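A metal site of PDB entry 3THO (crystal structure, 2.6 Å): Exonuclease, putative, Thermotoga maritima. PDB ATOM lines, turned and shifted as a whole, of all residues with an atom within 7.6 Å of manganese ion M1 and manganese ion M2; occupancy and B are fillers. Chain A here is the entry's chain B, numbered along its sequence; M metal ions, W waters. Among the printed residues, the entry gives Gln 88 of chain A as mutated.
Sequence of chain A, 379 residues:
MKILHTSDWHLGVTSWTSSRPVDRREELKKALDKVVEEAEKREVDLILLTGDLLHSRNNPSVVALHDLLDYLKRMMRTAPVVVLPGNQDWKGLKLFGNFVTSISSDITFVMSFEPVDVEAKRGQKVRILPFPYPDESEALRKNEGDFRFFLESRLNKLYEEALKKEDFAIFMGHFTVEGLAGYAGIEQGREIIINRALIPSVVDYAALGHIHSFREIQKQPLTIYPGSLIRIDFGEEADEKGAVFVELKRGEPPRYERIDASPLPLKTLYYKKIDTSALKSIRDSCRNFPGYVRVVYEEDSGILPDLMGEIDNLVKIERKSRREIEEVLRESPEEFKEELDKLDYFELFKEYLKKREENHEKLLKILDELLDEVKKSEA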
ATOM      1  N   SER A   7      34.501   0.456   1.384  1.00  0.00           N
ATOM      2  CA  SER A   7      33.624   0.006   2.453  1.00  0.00           C
ATOM      3  C   SER A   7      32.861   1.185   3.074  1.00  0.00           C
ATOM      4  O   SER A   7      33.163   2.343   2.808  1.00  0.00           O
ATOM      5  CB  SER A   7      34.512  -0.626   3.556  1.00  0.00           C
ATOM      6  OG  SER A   7      33.772  -1.376   4.508  1.00  0.00           O
ATOM      7  N   ASP A   8      31.870   0.849   3.904  1.00  0.00           N
ATOM      8  CA  ASP A   8      31.199   1.808   4.761  1.00  0.00           C
ATOM      9  C   ASP A   8      30.558   3.014   4.031  1.00  0.00           C
ATOM     10  O   ASP A   8      30.435   4.099   4.601  1.00  0.00           O
ATOM     11  CB  ASP A   8      32.152   2.253   5.891  1.00  0.00           C
ATOM     12  CG  ASP A   8      32.583   1.079   6.769  1.00  0.00           C
ATOM     13  OD1 ASP A   8      33.555   0.340   6.415  1.00  0.00           O
ATOM     14  OD2 ASP A   8      31.948   0.874   7.841  1.00  0.00           O
ATOM     15  N   TRP A   9      30.137   2.775   2.798  1.00  0.00           N
ATOM     16  CA  TRP A   9      29.439   3.745   1.971  1.00  0.00           C
ATOM     17  C   TRP A   9      28.263   4.426   2.695  1.00  0.00           C
ATOM     18  O   TRP A   9      28.132   5.652   2.675  1.00  0.00           O
ATOM     19  CB  TRP A   9      28.883   3.078   0.716  1.00  0.00           C
ATOM     20  CG  TRP A   9      29.934   2.457  -0.142  1.00  0.00           C
ATOM     21  CD1 TRP A   9      31.278   2.469   0.069  1.00  0.00           C
ATOM     22  CD2 TRP A   9      29.723   1.761  -1.389  1.00  0.00           C
ATOM     23  NE1 TRP A   9      31.933   1.816  -0.955  1.00  0.00           N
ATOM     24  CE2 TRP A   9      31.001   1.361  -1.849  1.00  0.00           C
ATOM     25  CE3 TRP A   9      28.586   1.423  -2.141  1.00  0.00           C
ATOM     26  CZ2 TRP A   9      31.167   0.644  -3.045  1.00  0.00           C
ATOM     27  CZ3 TRP A   9      28.756   0.711  -3.323  1.00  0.00           C
ATOM     28  CH2 TRP A   9      30.047   0.324  -3.769  1.00  0.00           C
ATOM     29  N   HIS A  10      27.386   3.620   3.278  1.00  0.00           N
ATOM     30  CA  HIS A  10      26.219   4.158   3.987  1.00  0.00           C
ATOM     31  C   HIS A  10      25.205   4.862   3.053  1.00  0.00           C
ATOM     32  O   HIS A  10      24.534   5.795   3.466  1.00  0.00           O
ATOM     33  CB  HIS A  10      26.666   5.117   5.086  1.00  0.00           C
ATOM     34  CG  HIS A  10      27.177   4.433   6.316  1.00  0.00           C
ATOM     35  ND1 HIS A  10      26.370   4.121   7.390  1.00  0.00           N
ATOM     36  CD2 HIS A  10      28.411   3.989   6.648  1.00  0.00           C
ATOM     37  CE1 HIS A  10      27.078   3.531   8.333  1.00  0.00           C
ATOM     38  NE2 HIS A  10      28.338   3.439   7.903  1.00  0.00           N
ATOM     39  N   THR A  50      33.538  -4.369   1.788  1.00  0.00           N
ATOM     40  CA  THR A  50      33.462  -4.995   3.100  1.00  0.00           C
ATOM     41  C   THR A  50      32.353  -4.495   4.060  1.00  0.00           C
ATOM     42  O   THR A  50      32.556  -4.474   5.290  1.00  0.00           O
ATOM     43  CB  THR A  50      34.820  -4.922   3.824  1.00  0.00           C
ATOM     44  OG1 THR A  50      35.338  -3.593   3.721  1.00  0.00           O
ATOM     45  CG2 THR A  50      35.844  -5.916   3.213  1.00  0.00           C
ATOM     46  N   GLY A  51      31.212  -4.073   3.520  1.00  0.00           N
ATOM     47  CA  GLY A  51      30.001  -3.920   4.324  1.00  0.00           C
ATOM     48  C   GLY A  51      29.555  -2.505   4.679  1.00  0.00           C
ATOM     49  O   GLY A  51      30.317  -1.535   4.499  1.00  0.00           O
ATOM     50  N   ASP A  52      28.327  -2.382   5.206  1.00  0.00           N
ATOM     51  CA  ASP A  52      27.652  -1.095   5.416  1.00  0.00           C
ATOM     52  C   ASP A  52      27.654  -0.240   4.146  1.00  0.00           C
ATOM     53  O   ASP A  52      27.969   0.947   4.180  1.00  0.00           O
ATOM     54  CB  ASP A  52      28.276  -0.321   6.571  1.00  0.00           C
ATOM     55  CG  ASP A  52      28.167  -1.045   7.894  1.00  0.00           C
ATOM     56  OD1 ASP A  52      27.329  -1.974   8.011  1.00  0.00           O
ATOM     57  OD2 ASP A  52      28.903  -0.674   8.827  1.00  0.00           O
ATOM     58  N   LEU A  53      27.321  -0.882   3.027  1.00  0.00           N
ATOM     59  CA  LEU A  53      27.146  -0.174   1.766  1.00  0.00           C
ATOM     60  C   LEU A  53      25.818   0.596   1.808  1.00  0.00           C
ATOM     61  O   LEU A  53      25.663   1.673   1.215  1.00  0.00           O
ATOM     62  CB  LEU A  53      27.156  -1.180   0.599  1.00  0.00           C
ATOM     63  CG  LEU A  53      28.357  -2.118   0.493  1.00  0.00           C
ATOM     64  CD1 LEU A  53      28.262  -2.976  -0.767  1.00  0.00           C
ATOM     65  CD2 LEU A  53      29.675  -1.327   0.486  1.00  0.00           C
ATOM     66  N   LEU A  54      24.841   0.019   2.523  1.00  0.00           N
ATOM     67  CA  LEU A  54      23.580   0.684   2.821  1.00  0.00           C
ATOM     68  C   LEU A  54      23.625   1.255   4.220  1.00  0.00           C
ATOM     69  O   LEU A  54      24.415   0.812   5.062  1.00  0.00           O
ATOM     70  CB  LEU A  54      22.424  -0.296   2.728  1.00  0.00           C
ATOM     71  CG  LEU A  54      22.204  -0.745   1.286  1.00  0.00           C
ATOM     72  CD1 LEU A  54      21.263  -1.950   1.230  1.00  0.00           C
ATOM     73  CD2 LEU A  54      21.674   0.424   0.464  1.00  0.00           C
ATOM     74  N   HIS A  55      22.779   2.244   4.482  1.00  0.00           N
ATOM     75  CA  HIS A  55      22.767   2.883   5.788  1.00  0.00           C
ATOM     76  C   HIS A  55      21.796   2.220   6.761  1.00  0.00           C
ATOM     77  O   HIS A  55      22.064   2.128   7.983  1.00  0.00           O
ATOM     78  CB  HIS A  55      22.419   4.375   5.663  1.00  0.00           C
ATOM     79  CG  HIS A  55      22.413   5.072   6.979  1.00  0.00           C
ATOM     80  ND1 HIS A  55      23.554   5.249   7.723  1.00  0.00           N
ATOM     81  CD2 HIS A  55      21.397   5.577   7.715  1.00  0.00           C
ATOM     82  CE1 HIS A  55      23.248   5.869   8.856  1.00  0.00           C
ATOM     83  NE2 HIS A  55      21.945   6.083   8.872  1.00  0.00           N
ATOM     84  N   PRO A  85      28.585  -8.317   3.516  1.00  0.00           N
ATOM     85  CA  PRO A  85      27.622  -7.404   4.163  1.00  0.00           C
ATOM     86  C   PRO A  85      27.973  -7.086   5.624  1.00  0.00           C
ATOM     87  O   PRO A  85      28.518  -7.942   6.321  1.00  0.00           O
ATOM     88  CB  PRO A  85      26.294  -8.191   4.093  1.00  0.00           C
ATOM     89  CG  PRO A  85      26.489  -9.140   2.923  1.00  0.00           C
ATOM     90  CD  PRO A  85      27.952  -9.531   2.972  1.00  0.00           C
ATOM     91  N   GLY A  86      27.658  -5.874   6.069  1.00  0.00           N
ATOM     92  CA  GLY A  86      27.904  -5.451   7.437  1.00  0.00           C
ATOM     93  C   GLY A  86      26.645  -5.472   8.273  1.00  0.00           C
ATOM     94  O   GLY A  86      25.546  -5.803   7.785  1.00  0.00           O
ATOM     95  N   ASN A  87      26.779  -5.121   9.555  1.00  0.00           N
ATOM     96  CA  ASN A  87      25.659  -5.085  10.491  1.00  0.00           C
ATOM     97  C   ASN A  87      24.566  -4.078  10.103  1.00  0.00           C
ATOM     98  O   ASN A  87      23.404  -4.295  10.367  1.00  0.00           O
ATOM     99  CB  ASN A  87      26.168  -4.768  11.897  1.00  0.00           C
ATOM    100  CG  ASN A  87      26.912  -3.454  11.943  1.00  0.00           C
ATOM    101  OD1 ASN A  87      27.848  -3.251  11.157  1.00  0.00           O
ATOM    102  ND2 ASN A  87      26.498  -2.542  12.812  1.00  0.00           N
ATOM    103  N   GLN A  88      24.953  -2.970   9.478  1.00  0.00           N
ATOM    104  CA  GLN A  88      23.963  -1.982   9.063  1.00  0.00           C
ATOM    105  C   GLN A  88      23.354  -2.227   7.680  1.00  0.00           C
ATOM    106  O   GLN A  88      22.426  -1.521   7.275  1.00  0.00           O
ATOM    107  CB  GLN A  88      24.568  -0.586   9.100  1.00  0.00           C
ATOM    108  CG  GLN A  88      24.535   0.030  10.473  1.00  0.00           C
ATOM    109  CD  GLN A  88      25.590   1.082  10.644  1.00  0.00           C
ATOM    110  OE1 GLN A  88      25.285   2.283  10.629  1.00  0.00           O
ATOM    111  NE2 GLN A  88      26.852   0.648  10.827  1.00  0.00           N
ATOM    112  N   ASP A  89      23.869  -3.198   6.928  1.00  0.00           N
ATOM    113  CA  ASP A  89      23.268  -3.471   5.621  1.00  0.00           C
ATOM    114  C   ASP A  89      21.888  -4.092   5.807  1.00  0.00           C
ATOM    115  O   ASP A  89      21.674  -4.926   6.679  1.00  0.00           O
ATOM    116  CB  ASP A  89      24.172  -4.364   4.760  1.00  0.00           C
ATOM    117  CG  ASP A  89      25.357  -3.587   4.132  1.00  0.00           C
ATOM    118  OD1 ASP A  89      25.137  -2.474   3.581  1.00  0.00           O
ATOM    119  OD2 ASP A  89      26.511  -4.087   4.188  1.00  0.00           O
ATOM    120  N   TYR A 133      30.180  -9.657  10.786  1.00  0.00           N
ATOM    121  CA  TYR A 133      30.001  -8.986  12.054  1.00  0.00           C
ATOM    122  C   TYR A 133      29.445  -9.961  13.105  1.00  0.00           C
ATOM    123  O   TYR A 133      28.534 -10.722  12.816  1.00  0.00           O
ATOM    124  CB  TYR A 133      29.032  -7.824  11.859  1.00  0.00           C
ATOM    125  CG  TYR A 133      28.836  -6.987  13.083  1.00  0.00           C
ATOM    126  CD1 TYR A 133      29.761  -6.002  13.408  1.00  0.00           C
ATOM    127  CD2 TYR A 133      27.725  -7.165  13.912  1.00  0.00           C
ATOM    128  CE1 TYR A 133      29.600  -5.195  14.526  1.00  0.00           C
ATOM    129  CE2 TYR A 133      27.551  -6.377  15.032  1.00  0.00           C
ATOM    130  CZ  TYR A 133      28.491  -5.383  15.335  1.00  0.00           C
ATOM    131  OH  TYR A 133      28.336  -4.581  16.446  1.00  0.00           O
ATOM    132  N   HIS A 174      34.276  -7.859   9.078  1.00  0.00           N
ATOM    133  CA  HIS A 174      33.488  -6.665   9.417  1.00  0.00           C
ATOM    134  C   HIS A 174      33.253  -6.643  10.917  1.00  0.00           C
ATOM    135  O   HIS A 174      32.371  -7.345  11.421  1.00  0.00           O
ATOM    136  CB  HIS A 174      32.169  -6.631   8.654  1.00  0.00           C
ATOM    137  CG  HIS A 174      31.456  -5.311   8.724  1.00  0.00           C
ATOM    138  ND1 HIS A 174      31.530  -4.360   7.741  1.00  0.00           N
ATOM    139  CD2 HIS A 174      30.664  -4.795   9.700  1.00  0.00           C
ATOM    140  CE1 HIS A 174      30.809  -3.305   8.087  1.00  0.00           C
ATOM    141  NE2 HIS A 174      30.274  -3.543   9.260  1.00  0.00           N
ATOM    142  N   PHE A 175      34.059  -5.842  11.611  1.00  0.00           N
ATOM    143  CA  PHE A 175      34.074  -5.780  13.082  1.00  0.00           C
ATOM    144  C   PHE A 175      35.091  -4.738  13.557  1.00  0.00           C
ATOM    145  O   PHE A 175      35.844  -4.137  12.744  1.00  0.00           O
ATOM    146  CB  PHE A 175      34.428  -7.140  13.698  1.00  0.00           C
ATOM    147  CG  PHE A 175      35.718  -7.702  13.181  1.00  0.00           C
ATOM    148  CD1 PHE A 175      36.917  -7.332  13.753  1.00  0.00           C
ATOM    149  CD2 PHE A 175      35.740  -8.570  12.088  1.00  0.00           C
ATOM    150  CE1 PHE A 175      38.134  -7.831  13.256  1.00  0.00           C
ATOM    151  CE2 PHE A 175      36.951  -9.082  11.582  1.00  0.00           C
ATOM    152  CZ  PHE A 175      38.148  -8.703  12.174  1.00  0.00           C
ATOM    153  N   THR A 176      35.114  -4.524  14.860  1.00  0.00           N
ATOM    154  CA  THR A 176      35.990  -3.536  15.488  1.00  0.00           C
ATOM    155  C   THR A 176      37.196  -4.253  16.088  1.00  0.00           C
ATOM    156  O   THR A 176      37.014  -5.194  16.858  1.00  0.00           O
ATOM    157  CB  THR A 176      35.234  -2.855  16.645  1.00  0.00           C
ATOM    158  OG1 THR A 176      34.054  -2.192  16.149  1.00  0.00           O
ATOM    159  CG2 THR A 176      36.132  -1.880  17.418  1.00  0.00           C
ATOM    160  N   GLU A 191      29.797  -4.066  21.628  1.00  0.00           N
ATOM    161  CA  GLU A 191      30.274  -4.901  20.525  1.00  0.00           C
ATOM    162  C   GLU A 191      31.200  -5.974  21.069  1.00  0.00           C
ATOM    163  O   GLU A 191      31.816  -5.799  22.122  1.00  0.00           O
ATOM    164  CB  GLU A 191      31.054  -4.071  19.497  1.00  0.00           C
ATOM    165  CG  GLU A 191      30.220  -3.212  18.549  1.00  0.00           C
ATOM    166  CD  GLU A 191      31.071  -2.636  17.414  1.00  0.00           C
ATOM    167  OE1 GLU A 191      32.126  -3.237  17.099  1.00  0.00           O
ATOM    168  OE2 GLU A 191      30.695  -1.594  16.826  1.00  0.00           O
ATOM    169  N   GLY A 209      35.968  -3.714   7.202  1.00  0.00           N
ATOM    170  CA  GLY A 209      35.011  -2.620   7.149  1.00  0.00           C
ATOM    171  C   GLY A 209      34.356  -2.451   8.521  1.00  0.00           C
ATOM    172  O   GLY A 209      34.576  -3.301   9.413  1.00  0.00           O
ATOM    173  N   HIS A 210      33.571  -1.381   8.694  1.00  0.00           N
ATOM    174  CA  HIS A 210      32.761  -1.099   9.906  1.00  0.00           C
ATOM    175  C   HIS A 210      33.223   0.188  10.614  1.00  0.00           C
ATOM    176  O   HIS A 210      32.456   0.830  11.341  1.00  0.00           O
ATOM    177  CB  HIS A 210      32.742  -2.288  10.895  1.00  0.00           C
ATOM    178  CG  HIS A 210      31.899  -2.058  12.118  1.00  0.00           C
ATOM    179  ND1 HIS A 210      30.543  -1.892  12.087  1.00  0.00           N
ATOM    180  CD2 HIS A 210      32.267  -1.941  13.428  1.00  0.00           C
ATOM    181  CE1 HIS A 210      30.073  -1.701  13.314  1.00  0.00           C
ATOM    182  NE2 HIS A 210      31.095  -1.725  14.140  1.00  0.00           N
ATOM    183  N   ILE A 211      34.478   0.556  10.376  1.00  0.00           N
ATOM    184  CA  ILE A 211      35.152   1.702  11.001  1.00  0.00           C
ATOM    185  C   ILE A 211      35.316   2.779   9.922  1.00  0.00           C
ATOM    186  O   ILE A 211      35.691   2.472   8.781  1.00  0.00           O
ATOM    187  CB  ILE A 211      36.544   1.270  11.527  1.00  0.00           C
ATOM    188  CG1 ILE A 211      36.403   0.292  12.698  1.00  0.00           C
ATOM    189  CG2 ILE A 211      37.385   2.466  11.926  1.00  0.00           C
ATOM    190  CD1 ILE A 211      35.968   0.929  13.949  1.00  0.00           C
ATOM    191  N   HIS A 212      35.032   4.032  10.268  1.00  0.00           N
ATOM    192  CA  HIS A 212      34.864   5.065   9.233  1.00  0.00           C
ATOM    193  C   HIS A 212      36.136   5.805   8.903  1.00  0.00           C
ATOM    194  O   HIS A 212      36.219   6.474   7.866  1.00  0.00           O
ATOM    195  CB  HIS A 212      33.758   6.065   9.610  1.00  0.00           C
ATOM    196  CG  HIS A 212      32.418   5.429   9.899  1.00  0.00           C
ATOM    197  ND1 HIS A 212      31.386   6.118  10.446  1.00  0.00           N
ATOM    198  CD2 HIS A 212      31.996   4.149   9.700  1.00  0.00           C
ATOM    199  CE1 HIS A 212      30.336   5.307  10.592  1.00  0.00           C
ATOM    200  NE2 HIS A 212      30.680   4.116  10.140  1.00  0.00           N
ATOM    201  N   SER A 228      35.083   5.382   5.627  1.00  0.00           N
ATOM    202  CA  SER A 228      33.963   5.840   4.810  1.00  0.00           C
ATOM    203  C   SER A 228      34.390   6.749   3.645  1.00  0.00           C
ATOM    204  O   SER A 228      35.560   7.077   3.494  1.00  0.00           O
ATOM    205  CB  SER A 228      32.908   6.506   5.693  1.00  0.00           C
ATOM    206  OG  SER A 228      33.491   7.483   6.522  1.00  0.00           O
ATOM    207  N   ILE A 232      30.647  11.445   8.266  1.00  0.00           N
ATOM    208  CA  ILE A 232      29.279  11.127   8.601  1.00  0.00           C
ATOM    209  C   ILE A 232      28.789  11.989   9.760  1.00  0.00           C
ATOM    210  O   ILE A 232      27.631  12.413   9.761  1.00  0.00           O
ATOM    211  CB  ILE A 232      29.112   9.589   8.825  1.00  0.00           C
ATOM    212  CG1 ILE A 232      29.515   8.853   7.530  1.00  0.00           C
ATOM    213  CG2 ILE A 232      27.699   9.244   9.226  1.00  0.00           C
ATOM    214  CD1 ILE A 232      28.965   7.475   7.358  1.00  0.00           C
HETATM  215 MN    MN M   1      29.490  -1.941  10.488  1.00  0.00          MN
HETATM  216 MN    MN M   2      29.857   1.585   9.252  1.00  0.00          MN
HETATM  217  O   HOH W   1      30.314   1.606  12.437  1.00  0.00           O
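OD2 of Asp 89 is in hydrogen-bond range of N of Asp 52 (2.7 Å). N of His 10 sits at hydrogen-bond distance from O of Asp 52 (2.9 Å). A ring nitrogen (NE2) of His 210 lies within hydrogen-bond range of the side-chain carboxylate of Glu 191, at 2.7 Å. ND1 of His 10 lies within hydrogen-bond range of ND1 of His 55 (3.1 Å). OG of Ser 7 lies within hydrogen-bond range of OD1 of Asp 8. A ring nitrogen (NE2) of His 212 is in hydrogen-bond range of a ring nitrogen (NE2) of His 10 (3.3 Å). The side-chain carboxylate of Asp 52 sits at hydrogen-bond distance from the backbone NH of Gln 88, at 3.0 Å. O of Asp 52 lies within hydrogen-bond range of N of Trp 9 (3.2 Å).
Gln 88 touches manganese ion M1. Of the 26 residues printed, 5 come within 4 Å of manganese ion M1. The nearest printed residue that does not touch manganese ion M1 is Asp 8 (4.6 Å).
Gln 88 touches manganese ion M2. Within 4 Å of manganese ion M2: Asp 8, His 10, Asp 52, Gln 88, His 210 and His 212.
Manganese ion M1 is bound by a ring nitrogen (ND1) of His 210 (1.9 Å), a ring nitrogen (NE2) of His 174 (2.2 Å), the side-chain carboxylate (OD2) of Asp 52 (2.2 Å) and the side-chain amide oxygen (OD1) of Asn 87 (2.2 Å).
Manganese ion M2 is bound by OD2 of Asp 52 (2.5 Å) and OD2 of Asp 8 (2.6 Å). Manganese ion M2 has two donor atoms within binding distance. Slightly farther from manganese ion M2 lies a ring nitrogen (NE2) of His 10 (2.8 Å). Slightly farther from manganese ion M2 lies a ring nitrogen (NE2) of His 212 (2.8 Å).
Water W1 bridges the backbone carbonyl oxygen (O) of His 210 (2.5 Å) and a ring nitrogen (NE2) of His 212 (3.4 Å).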
